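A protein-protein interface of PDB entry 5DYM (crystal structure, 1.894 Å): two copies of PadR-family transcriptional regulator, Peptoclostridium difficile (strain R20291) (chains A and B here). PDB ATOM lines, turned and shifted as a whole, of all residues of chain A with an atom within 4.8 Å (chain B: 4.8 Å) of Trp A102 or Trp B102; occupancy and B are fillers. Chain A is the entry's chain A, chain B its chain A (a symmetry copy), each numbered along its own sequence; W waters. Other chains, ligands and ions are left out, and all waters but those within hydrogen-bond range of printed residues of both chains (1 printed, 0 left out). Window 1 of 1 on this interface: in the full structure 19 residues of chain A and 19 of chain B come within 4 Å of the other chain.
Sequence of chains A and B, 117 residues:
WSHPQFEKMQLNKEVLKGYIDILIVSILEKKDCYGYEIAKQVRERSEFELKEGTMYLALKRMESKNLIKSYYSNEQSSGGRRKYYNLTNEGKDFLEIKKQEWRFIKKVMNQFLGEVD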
ATOM      1  N   LYS A  98      24.791   5.722   6.447  1.00  0.00           N
ATOM      2  CA  LYS A  98      24.997   7.021   7.079  1.00  0.00           C
ATOM      3  C   LYS A  98      24.427   7.064   8.491  1.00  0.00           C
ATOM      4  O   LYS A  98      25.054   7.615   9.395  1.00  0.00           O
ATOM      5  CB  LYS A  98      24.378   8.141   6.237  1.00  0.00           C
ATOM      6  CG  LYS A  98      25.071   8.340   4.902  1.00  0.00           C
ATOM      7  CD  LYS A  98      26.512   8.771   5.092  1.00  0.00           C
ATOM      8  CE  LYS A  98      27.460   7.838   4.371  1.00  0.00           C
ATOM      9  NZ  LYS A  98      28.836   8.395   4.318  1.00  0.00           N
ATOM     10  N   LYS A  99      23.244   6.488   8.680  1.00  0.00           N
ATOM     11  CA  LYS A  99      22.621   6.456   9.994  1.00  0.00           C
ATOM     12  C   LYS A  99      23.517   5.703  10.984  1.00  0.00           C
ATOM     13  O   LYS A  99      23.719   6.143  12.118  1.00  0.00           O
ATOM     14  CB  LYS A  99      21.245   5.794   9.924  1.00  0.00           C
ATOM     15  CG  LYS A  99      20.116   6.680   9.419  1.00  0.00           C
ATOM     16  CD  LYS A  99      18.778   5.946   9.565  1.00  0.00           C
ATOM     17  CE  LYS A  99      17.628   6.769   9.006  1.00  0.00           C
ATOM     18  NZ  LYS A  99      16.458   5.897   8.668  1.00  0.00           N
ATOM     19  N   GLN A 100      24.048   4.569  10.540  1.00  0.00           N
ATOM     20  CA  GLN A 100      24.966   3.777  11.363  1.00  0.00           C
ATOM     21  C   GLN A 100      26.237   4.550  11.706  1.00  0.00           C
ATOM     22  O   GLN A 100      26.671   4.573  12.859  1.00  0.00           O
ATOM     23  CB  GLN A 100      25.337   2.477  10.658  1.00  0.00           C
ATOM     24  CG  GLN A 100      24.201   1.475  10.567  1.00  0.00           C
ATOM     25  CD  GLN A 100      24.581   0.242   9.764  1.00  0.00           C
ATOM     26  OE1 GLN A 100      25.739   0.073   9.370  1.00  0.00           O
ATOM     27  NE2 GLN A 100      23.605  -0.627   9.513  1.00  0.00           N
ATOM     28  N   GLU A 101      26.838   5.180  10.703  1.00  0.00           N
ATOM     29  CA  GLU A 101      28.059   5.943  10.924  1.00  0.00           C
ATOM     30  C   GLU A 101      27.814   7.112  11.866  1.00  0.00           C
ATOM     31  O   GLU A 101      28.680   7.460  12.667  1.00  0.00           O
ATOM     32  CB  GLU A 101      28.635   6.444   9.601  1.00  0.00           C
ATOM     33  CG  GLU A 101      29.228   5.333   8.749  1.00  0.00           C
ATOM     34  CD  GLU A 101      29.762   5.832   7.418  1.00  0.00           C
ATOM     35  OE1 GLU A 101      29.712   7.054   7.177  1.00  0.00           O
ATOM     36  OE2 GLU A 101      30.236   4.998   6.614  1.00  0.00           O
ATOM     37  N   TRP A 102      26.630   7.712  11.781  1.00  0.00           N
ATOM     38  CA  TRP A 102      26.321   8.850  12.635  1.00  0.00           C
ATOM     39  C   TRP A 102      26.236   8.441  14.106  1.00  0.00           C
ATOM     40  O   TRP A 102      26.772   9.132  14.970  1.00  0.00           O
ATOM     41  CB  TRP A 102      25.018   9.520  12.206  1.00  0.00           C
ATOM     42  CG  TRP A 102      24.581  10.598  13.152  1.00  0.00           C
ATOM     43  CD1 TRP A 102      23.440  10.618  13.892  1.00  0.00           C
ATOM     44  CD2 TRP A 102      25.292  11.804  13.475  1.00  0.00           C
ATOM     45  NE1 TRP A 102      23.381  11.769  14.647  1.00  0.00           N
ATOM     46  CE2 TRP A 102      24.510  12.511  14.413  1.00  0.00           C
ATOM     47  CE3 TRP A 102      26.511  12.354  13.066  1.00  0.00           C
ATOM     48  CZ2 TRP A 102      24.907  13.738  14.948  1.00  0.00           C
ATOM     49  CZ3 TRP A 102      26.905  13.577  13.599  1.00  0.00           C
ATOM     50  CH2 TRP A 102      26.103  14.253  14.527  1.00  0.00           C
ATOM     51  N   ARG A 103      25.562   7.326  14.381  1.00  0.00           N
ATOM     52  CA  ARG A 103      25.423   6.832  15.751  1.00  0.00           C
ATOM     53  C   ARG A 103      26.806   6.621  16.376  1.00  0.00           C
ATOM     54  O   ARG A 103      27.052   7.015  17.515  1.00  0.00           O
ATOM     55  CB  ARG A 103      24.609   5.532  15.783  1.00  0.00           C
ATOM     56  CG  ARG A 103      23.103   5.730  15.589  1.00  0.00           C
ATOM     57  CD  ARG A 103      22.306   4.447  15.863  1.00  0.00           C
ATOM     58  NE  ARG A 103      22.360   3.493  14.755  1.00  0.00           N
ATOM     59  CZ  ARG A 103      21.539   3.511  13.704  1.00  0.00           C
ATOM     60  NH1 ARG A 103      20.591   4.436  13.617  1.00  0.00           N
ATOM     61  NH2 ARG A 103      21.664   2.605  12.738  1.00  0.00           N
ATOM     62  N   PHE A 104      27.703   6.023  15.600  1.00  0.00           N
ATOM     63  CA  PHE A 104      29.088   5.816  16.002  1.00  0.00           C
ATOM     64  C   PHE A 104      29.839   7.129  16.257  1.00  0.00           C
ATOM     65  O   PHE A 104      30.335   7.363  17.361  1.00  0.00           O
ATOM     66  CB  PHE A 104      29.803   4.996  14.933  1.00  0.00           C
ATOM     67  CG  PHE A 104      31.267   4.827  15.178  1.00  0.00           C
ATOM     68  CD1 PHE A 104      31.724   3.903  16.106  1.00  0.00           C
ATOM     69  CD2 PHE A 104      32.188   5.574  14.470  1.00  0.00           C
ATOM     70  CE1 PHE A 104      33.075   3.741  16.332  1.00  0.00           C
ATOM     71  CE2 PHE A 104      33.544   5.417  14.693  1.00  0.00           C
ATOM     72  CZ  PHE A 104      33.987   4.496  15.623  1.00  0.00           C
ATOM     73  N   ILE A 105      29.911   7.975  15.233  1.00  0.00           N
ATOM     74  CA  ILE A 105      30.618   9.255  15.299  1.00  0.00           C
ATOM     75  C   ILE A 105      30.144  10.152  16.442  1.00  0.00           C
ATOM     76  O   ILE A 105      30.957  10.751  17.160  1.00  0.00           O
ATOM     77  CB  ILE A 105      30.464  10.018  13.970  1.00  0.00           C
ATOM     78  CG1 ILE A 105      31.356   9.387  12.905  1.00  0.00           C
ATOM     79  CG2 ILE A 105      30.813  11.501  14.131  1.00  0.00           C
ATOM     80  CD1 ILE A 105      30.936   9.732  11.494  1.00  0.00           C
ATOM     81  N   LYS A 106      28.825  10.234  16.602  1.00  0.00           N
ATOM     82  CA  LYS A 106      28.191  11.103  17.588  1.00  0.00           C
ATOM     83  C   LYS A 106      28.633  10.778  19.012  1.00  0.00           C
ATOM     84  O   LYS A 106      28.765  11.668  19.860  1.00  0.00           O
ATOM     85  CB  LYS A 106      26.672  10.979  17.477  1.00  0.00           C
ATOM     86  CG  LYS A 106      25.885  11.990  18.259  1.00  0.00           C
ATOM     87  CD  LYS A 106      24.388  11.759  18.062  1.00  0.00           C
ATOM     88  CE  LYS A 106      24.035  10.283  18.222  1.00  0.00           C
ATOM     89  NZ  LYS A 106      22.632   9.990  17.807  1.00  0.00           N
ATOM     90  N   LYS A 107      28.854   9.492  19.255  1.00  0.00           N
ATOM     91  CA  LYS A 107      29.274   9.005  20.556  1.00  0.00           C
ATOM     92  C   LYS A 107      30.684   9.493  20.874  1.00  0.00           C
ATOM     93  O   LYS A 107      30.944  10.030  21.954  1.00  0.00           O
ATOM     94  CB  LYS A 107      29.207   7.479  20.586  1.00  0.00           C
ATOM     95  CG  LYS A 107      29.363   6.852  21.960  1.00  0.00           C
ATOM     96  CD  LYS A 107      29.092   5.355  21.896  1.00  0.00           C
ATOM     97  CE  LYS A 107      29.502   4.656  23.184  1.00  0.00           C
ATOM     98  NZ  LYS A 107      29.368   3.177  23.072  1.00  0.00           N
ATOM     99  N   MET A 109      32.588  11.976  19.284  1.00  0.00           N
ATOM    100  CA  MET A 109      32.768  13.414  19.282  1.00  0.00           C
ATOM    101  C   MET A 109      32.123  14.088  20.498  1.00  0.00           C
ATOM    102  O   MET A 109      32.621  15.112  20.962  1.00  0.00           O
ATOM    103  CB  MET A 109      32.229  14.021  17.984  1.00  0.00           C
ATOM    104  CG  MET A 109      33.061  13.684  16.754  1.00  0.00           C
ATOM    105  SD  MET A 109      34.811  14.103  16.959  1.00  0.00           S
ATOM    106  CE  MET A 109      35.513  12.474  17.191  1.00  0.00           C
ATOM    107  N   ASN A 110      31.040  13.518  21.028  1.00  0.00           N
ATOM    108  CA  ASN A 110      30.455  14.066  22.248  1.00  0.00           C
ATOM    109  C   ASN A 110      31.421  13.881  23.415  1.00  0.00           C
ATOM    110  O   ASN A 110      31.563  14.766  24.252  1.00  0.00           O
ATOM    111  CB  ASN A 110      29.099  13.421  22.567  1.00  0.00           C
ATOM    112  CG  ASN A 110      27.942  14.090  21.824  1.00  0.00           C
ATOM    113  OD1 ASN A 110      28.045  15.244  21.394  1.00  0.00           O
ATOM    114  ND2 ASN A 110      26.828  13.368  21.683  1.00  0.00           N
ATOM    115  N   LEU A 113      34.590  16.371  22.275  1.00  0.00           N
ATOM    116  CA  LEU A 113      34.354  17.778  21.951  1.00  0.00           C
ATOM    117  C   LEU A 113      33.228  18.397  22.772  1.00  0.00           C
ATOM    118  O   LEU A 113      33.068  19.619  22.787  1.00  0.00           O
ATOM    119  CB  LEU A 113      34.054  17.939  20.461  1.00  0.00           C
ATOM    120  CG  LEU A 113      35.174  17.497  19.522  1.00  0.00           C
ATOM    121  CD1 LEU A 113      34.715  17.551  18.075  1.00  0.00           C
ATOM    122  CD2 LEU A 113      36.418  18.362  19.736  1.00  0.00           C
ATOM    123  N   LYS B  98      36.824  23.179  15.750  1.00  0.00           N
ATOM    124  CA  LYS B  98      36.193  21.865  15.697  1.00  0.00           C
ATOM    125  C   LYS B  98      35.019  21.758  16.661  1.00  0.00           C
ATOM    126  O   LYS B  98      33.983  21.192  16.314  1.00  0.00           O
ATOM    127  CB  LYS B  98      37.211  20.759  15.995  1.00  0.00           C
ATOM    128  CG  LYS B  98      38.280  20.626  14.928  1.00  0.00           C
ATOM    129  CD  LYS B  98      37.678  20.225  13.596  1.00  0.00           C
ATOM    130  CE  LYS B  98      38.058  21.207  12.509  1.00  0.00           C
ATOM    131  NZ  LYS B  98      37.709  20.688  11.162  1.00  0.00           N
ATOM    132  N   LYS B  99      35.180  22.296  17.866  1.00  0.00           N
ATOM    133  CA  LYS B  99      34.113  22.267  18.854  1.00  0.00           C
ATOM    134  C   LYS B  99      32.880  23.007  18.322  1.00  0.00           C
ATOM    135  O   LYS B  99      31.749  22.533  18.453  1.00  0.00           O
ATOM    136  CB  LYS B  99      34.575  22.894  20.168  1.00  0.00           C
ATOM    137  CG  LYS B  99      35.418  21.998  21.063  1.00  0.00           C
ATOM    138  CD  LYS B  99      35.662  22.692  22.408  1.00  0.00           C
ATOM    139  CE  LYS B  99      36.561  21.860  23.309  1.00  0.00           C
ATOM    140  NZ  LYS B  99      37.213  22.713  24.354  1.00  0.00           N
ATOM    141  N   GLN B 100      33.115  24.169  17.723  1.00  0.00           N
ATOM    142  CA  GLN B 100      32.034  24.955  17.122  1.00  0.00           C
ATOM    143  C   GLN B 100      31.345  24.204  15.985  1.00  0.00           C
ATOM    144  O   GLN B 100      30.117  24.151  15.916  1.00  0.00           O
ATOM    145  CB  GLN B 100      32.562  26.288  16.603  1.00  0.00           C
ATOM    146  CG  GLN B 100      32.963  27.263  17.693  1.00  0.00           C
ATOM    147  CD  GLN B 100      33.584  28.533  17.134  1.00  0.00           C
ATOM    148  OE1 GLN B 100      33.607  28.745  15.918  1.00  0.00           O
ATOM    149  NE2 GLN B 100      34.093  29.384  18.020  1.00  0.00           N
ATOM    150  N   GLU B 101      32.138  23.625  15.090  1.00  0.00           N
ATOM    151  CA  GLU B 101      31.580  22.886  13.965  1.00  0.00           C
ATOM    152  C   GLU B 101      30.786  21.679  14.440  1.00  0.00           C
ATOM    153  O   GLU B 101      29.771  21.326  13.841  1.00  0.00           O
ATOM    154  CB  GLU B 101      32.682  22.447  13.002  1.00  0.00           C
ATOM    155  CG  GLU B 101      33.288  23.602  12.221  1.00  0.00           C
ATOM    156  CD  GLU B 101      34.409  23.163  11.296  1.00  0.00           C
ATOM    157  OE1 GLU B 101      34.685  21.949  11.229  1.00  0.00           O
ATOM    158  OE2 GLU B 101      35.013  24.037  10.633  1.00  0.00           O
ATOM    159  N   TRP B 102      31.237  21.052  15.522  1.00  0.00           N
ATOM    160  CA  TRP B 102      30.545  19.877  16.032  1.00  0.00           C
ATOM    161  C   TRP B 102      29.158  20.232  16.568  1.00  0.00           C
ATOM    162  O   TRP B 102      28.190  19.525  16.292  1.00  0.00           O
ATOM    163  CB  TRP B 102      31.362  19.190  17.123  1.00  0.00           C
ATOM    164  CG  TRP B 102      30.619  18.068  17.785  1.00  0.00           C
ATOM    165  CD1 TRP B 102      30.256  17.993  19.094  1.00  0.00           C
ATOM    166  CD2 TRP B 102      30.129  16.870  17.162  1.00  0.00           C
ATOM    167  NE1 TRP B 102      29.584  16.815  19.336  1.00  0.00           N
ATOM    168  CE2 TRP B 102      29.487  16.111  18.163  1.00  0.00           C
ATOM    169  CE3 TRP B 102      30.167  16.367  15.857  1.00  0.00           C
ATOM    170  CZ2 TRP B 102      28.889  14.876  17.902  1.00  0.00           C
ATOM    171  CZ3 TRP B 102      29.572  15.136  15.598  1.00  0.00           C
ATOM    172  CH2 TRP B 102      28.945  14.407  16.617  1.00  0.00           C
ATOM    173  N   ARG B 103      29.069  21.319  17.332  1.00  0.00           N
ATOM    174  CA  ARG B 103      27.792  21.761  17.892  1.00  0.00           C
ATOM    175  C   ARG B 103      26.775  21.985  16.768  1.00  0.00           C
ATOM    176  O   ARG B 103      25.625  21.558  16.860  1.00  0.00           O
ATOM    177  CB  ARG B 103      27.972  23.038  18.723  1.00  0.00           C
ATOM    178  CG  ARG B 103      28.614  22.808  20.094  1.00  0.00           C
ATOM    179  CD  ARG B 103      28.559  24.060  20.981  1.00  0.00           C
ATOM    180  NE  ARG B 103      29.575  25.053  20.631  1.00  0.00           N
ATOM    181  CZ  ARG B 103      30.823  25.050  21.099  1.00  0.00           C
ATOM    182  NH1 ARG B 103      31.215  24.105  21.945  1.00  0.00           N
ATOM    183  NH2 ARG B 103      31.684  25.992  20.723  1.00  0.00           N
ATOM    184  N   PHE B 104      27.231  22.633  15.701  1.00  0.00           N
ATOM    185  CA  PHE B 104      26.426  22.862  14.508  1.00  0.00           C
ATOM    186  C   PHE B 104      25.991  21.560  13.822  1.00  0.00           C
ATOM    187  O   PHE B 104      24.795  21.300  13.671  1.00  0.00           O
ATOM    188  CB  PHE B 104      27.209  23.736  13.535  1.00  0.00           C
ATOM    189  CG  PHE B 104      26.533  23.935  12.218  1.00  0.00           C
ATOM    190  CD1 PHE B 104      25.486  24.837  12.093  1.00  0.00           C
ATOM    191  CD2 PHE B 104      26.950  23.236  11.102  1.00  0.00           C
ATOM    192  CE1 PHE B 104      24.861  25.026  10.878  1.00  0.00           C
ATOM    193  CE2 PHE B 104      26.326  23.421   9.881  1.00  0.00           C
ATOM    194  CZ  PHE B 104      25.283  24.319   9.769  1.00  0.00           C
ATOM    195  N   ILE B 105      26.968  20.753  13.417  1.00  0.00           N
ATOM    196  CA  ILE B 105      26.725  19.490  12.718  1.00  0.00           C
ATOM    197  C   ILE B 105      25.801  18.541  13.480  1.00  0.00           C
ATOM    198  O   ILE B 105      24.888  17.938  12.899  1.00  0.00           O
ATOM    199  CB  ILE B 105      28.059  18.770  12.440  1.00  0.00           C
ATOM    200  CG1 ILE B 105      28.790  19.461  11.294  1.00  0.00           C
ATOM    201  CG2 ILE B 105      27.838  17.291  12.104  1.00  0.00           C
ATOM    202  CD1 ILE B 105      30.270  19.154  11.260  1.00  0.00           C
ATOM    203  N   LYS B 106      26.046  18.419  14.783  1.00  0.00           N
ATOM    204  CA  LYS B 106      25.319  17.500  15.653  1.00  0.00           C
ATOM    205  C   LYS B 106      23.820  17.787  15.669  1.00  0.00           C
ATOM    206  O   LYS B 106      22.995  16.871  15.765  1.00  0.00           O
ATOM    207  CB  LYS B 106      25.877  17.590  17.072  1.00  0.00           C
ATOM    208  CG  LYS B 106      25.394  16.532  18.021  1.00  0.00           C
ATOM    209  CD  LYS B 106      26.025  16.731  19.397  1.00  0.00           C
ATOM    210  CE  LYS B 106      25.941  18.191  19.834  1.00  0.00           C
ATOM    211  NZ  LYS B 106      26.750  18.462  21.058  1.00  0.00           N
ATOM    212  N   LYS B 107      23.489  19.069  15.576  1.00  0.00           N
ATOM    213  CA  LYS B 107      22.109  19.521  15.581  1.00  0.00           C
ATOM    214  C   LYS B 107      21.395  19.058  14.315  1.00  0.00           C
ATOM    215  O   LYS B 107      20.302  18.491  14.371  1.00  0.00           O
ATOM    216  CB  LYS B 107      22.062  21.043  15.708  1.00  0.00           C
ATOM    217  CG  LYS B 107      20.689  21.625  15.992  1.00  0.00           C
ATOM    218  CD  LYS B 107      20.793  23.115  16.284  1.00  0.00           C
ATOM    219  CE  LYS B 107      19.424  23.779  16.302  1.00  0.00           C
ATOM    220  NZ  LYS B 107      19.532  25.258  16.449  1.00  0.00           N
ATOM    221  N   MET B 109      22.404  16.682  11.937  1.00  0.00           N
ATOM    222  CA  MET B 109      22.389  15.250  11.714  1.00  0.00           C
ATOM    223  C   MET B 109      21.441  14.518  12.669  1.00  0.00           C
ATOM    224  O   MET B 109      20.875  13.492  12.297  1.00  0.00           O
ATOM    225  CB  MET B 109      23.804  14.675  11.819  1.00  0.00           C
ATOM    226  CG  MET B 109      24.719  15.076  10.668  1.00  0.00           C
ATOM    227  SD  MET B 109      24.009  14.696   9.046  1.00  0.00           S
ATOM    228  CE  MET B 109      23.535  16.334   8.503  1.00  0.00           C
ATOM    229  N   ASN B 110      21.246  15.041  13.881  1.00  0.00           N
ATOM    230  CA  ASN B 110      20.272  14.436  14.784  1.00  0.00           C
ATOM    231  C   ASN B 110      18.864  14.604  14.218  1.00  0.00           C
ATOM    232  O   ASN B 110      18.046  13.695  14.303  1.00  0.00           O
ATOM    233  CB  ASN B 110      20.358  15.034  16.195  1.00  0.00           C
ATOM    234  CG  ASN B 110      21.432  14.362  17.053  1.00  0.00           C
ATOM    235  OD1 ASN B 110      21.840  13.227  16.786  1.00  0.00           O
ATOM    236  ND2 ASN B 110      21.881  15.060  18.098  1.00  0.00           N
ATOM    237  N   LEU B 113      19.064  12.238  10.769  1.00  0.00           N
ATOM    238  CA  LEU B 113      19.480  10.838  10.848  1.00  0.00           C
ATOM    239  C   LEU B 113      19.051  10.161  12.145  1.00  0.00           C
ATOM    240  O   LEU B 113      19.116   8.936  12.259  1.00  0.00           O
ATOM    241  CB  LEU B 113      20.995  10.721  10.682  1.00  0.00           C
ATOM    242  CG  LEU B 113      21.543  11.225   9.349  1.00  0.00           C
ATOM    243  CD1 LEU B 113      23.062  11.209   9.351  1.00  0.00           C
ATOM    244  CD2 LEU B 113      20.988  10.385   8.196  1.00  0.00           C
HETATM  245  O   HOH W   1      23.922  14.198  20.480  1.00  0.00           O
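The indole nitrogen (NE1) of Trp A102 is in hydrogen-bond range of the side-chain amide oxygen (OD1) of Asn B110 (3.0 Å). OD1 of Asn B110 lies close to NZ of Lys A106, at 3.5 Å. The side-chain amide oxygen of Asn A110 lies within hydrogen-bond range of the indole nitrogen of Trp B102. NZ of Lys B106 lies close to OD1 of Asn A110 (3.5 Å).
The backbone carbonyl oxygen (O) of Lys A106 is in hydrogen-bond range of the side-chain amide nitrogen (ND2) of Asn A110 (3.2 Å). The side-chain amide nitrogen of Asn B110 lies within hydrogen-bond range of the backbone carbonyl oxygen of Lys B106, 3.2 Å away.
Among the printed residues, pairs that only touch across the chains: Lys A99 with Leu B113, Trp A102 with Trp B102, Trp A102 with Lys B106, Trp A102 with Met B109, Trp A102 with Leu B113, Lys A106 with Trp B102, Met A109 with Trp B102, Leu A113 with Lys B99 and Leu A113 with Trp B102.
Lys A98 touches none of the printed residues of chain B. Printed residues of chain B within 4 Å of Lys A99: Leu B113. Of chain A, only Trp A102, Lys A106, Met A109, Asn A110 and Leu A113 come within 4 Å of Trp B102. Printed residues of chain A within 4 Å of Met B109: Trp A102. Of the printed residues of chain A, Leu B113 touches Lys A99 and Trp A102. The nearest residue of chain A that does not touch Trp B102 is Ile A105 (4.1 Å).
Hydrophobic or aromatic side chains of chain A within 4 Å of the printed part of chain B: Trp A102, Met A109 and Leu A113. Along chain A the printed residues that touch a printed residue of chain B span positions 99 to 113. Hydrophobic or aromatic side chains of chain B that line the printed part of chain A: Trp B102, Met B109 and Leu B113.
Trp A102 touches Lys B106, and with the chains exchanged Lys A106 touches Trp B102. Trp A102 touches Met B109, and with the chains exchanged Met A109 touches Trp B102. Trp A102 touches Asn B110, and with the chains exchanged Asn A110 touches Trp B102. Trp A102 touches Leu B113, and with the chains exchanged Leu A113 touches Trp B102. Positions printed for both chains: 98, 99, 100, 101, 102, 103, 104, 105, 106, 107, 109, 110 and 113. Of the 13 pairs that touch across the chains among the printed residues, 13 have their exchanged pair printed and touching as well.
Water W1 bridges ND2 of Asn A110 (3.3 Å) and ND2 of Asn B110 (3.3 Å).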
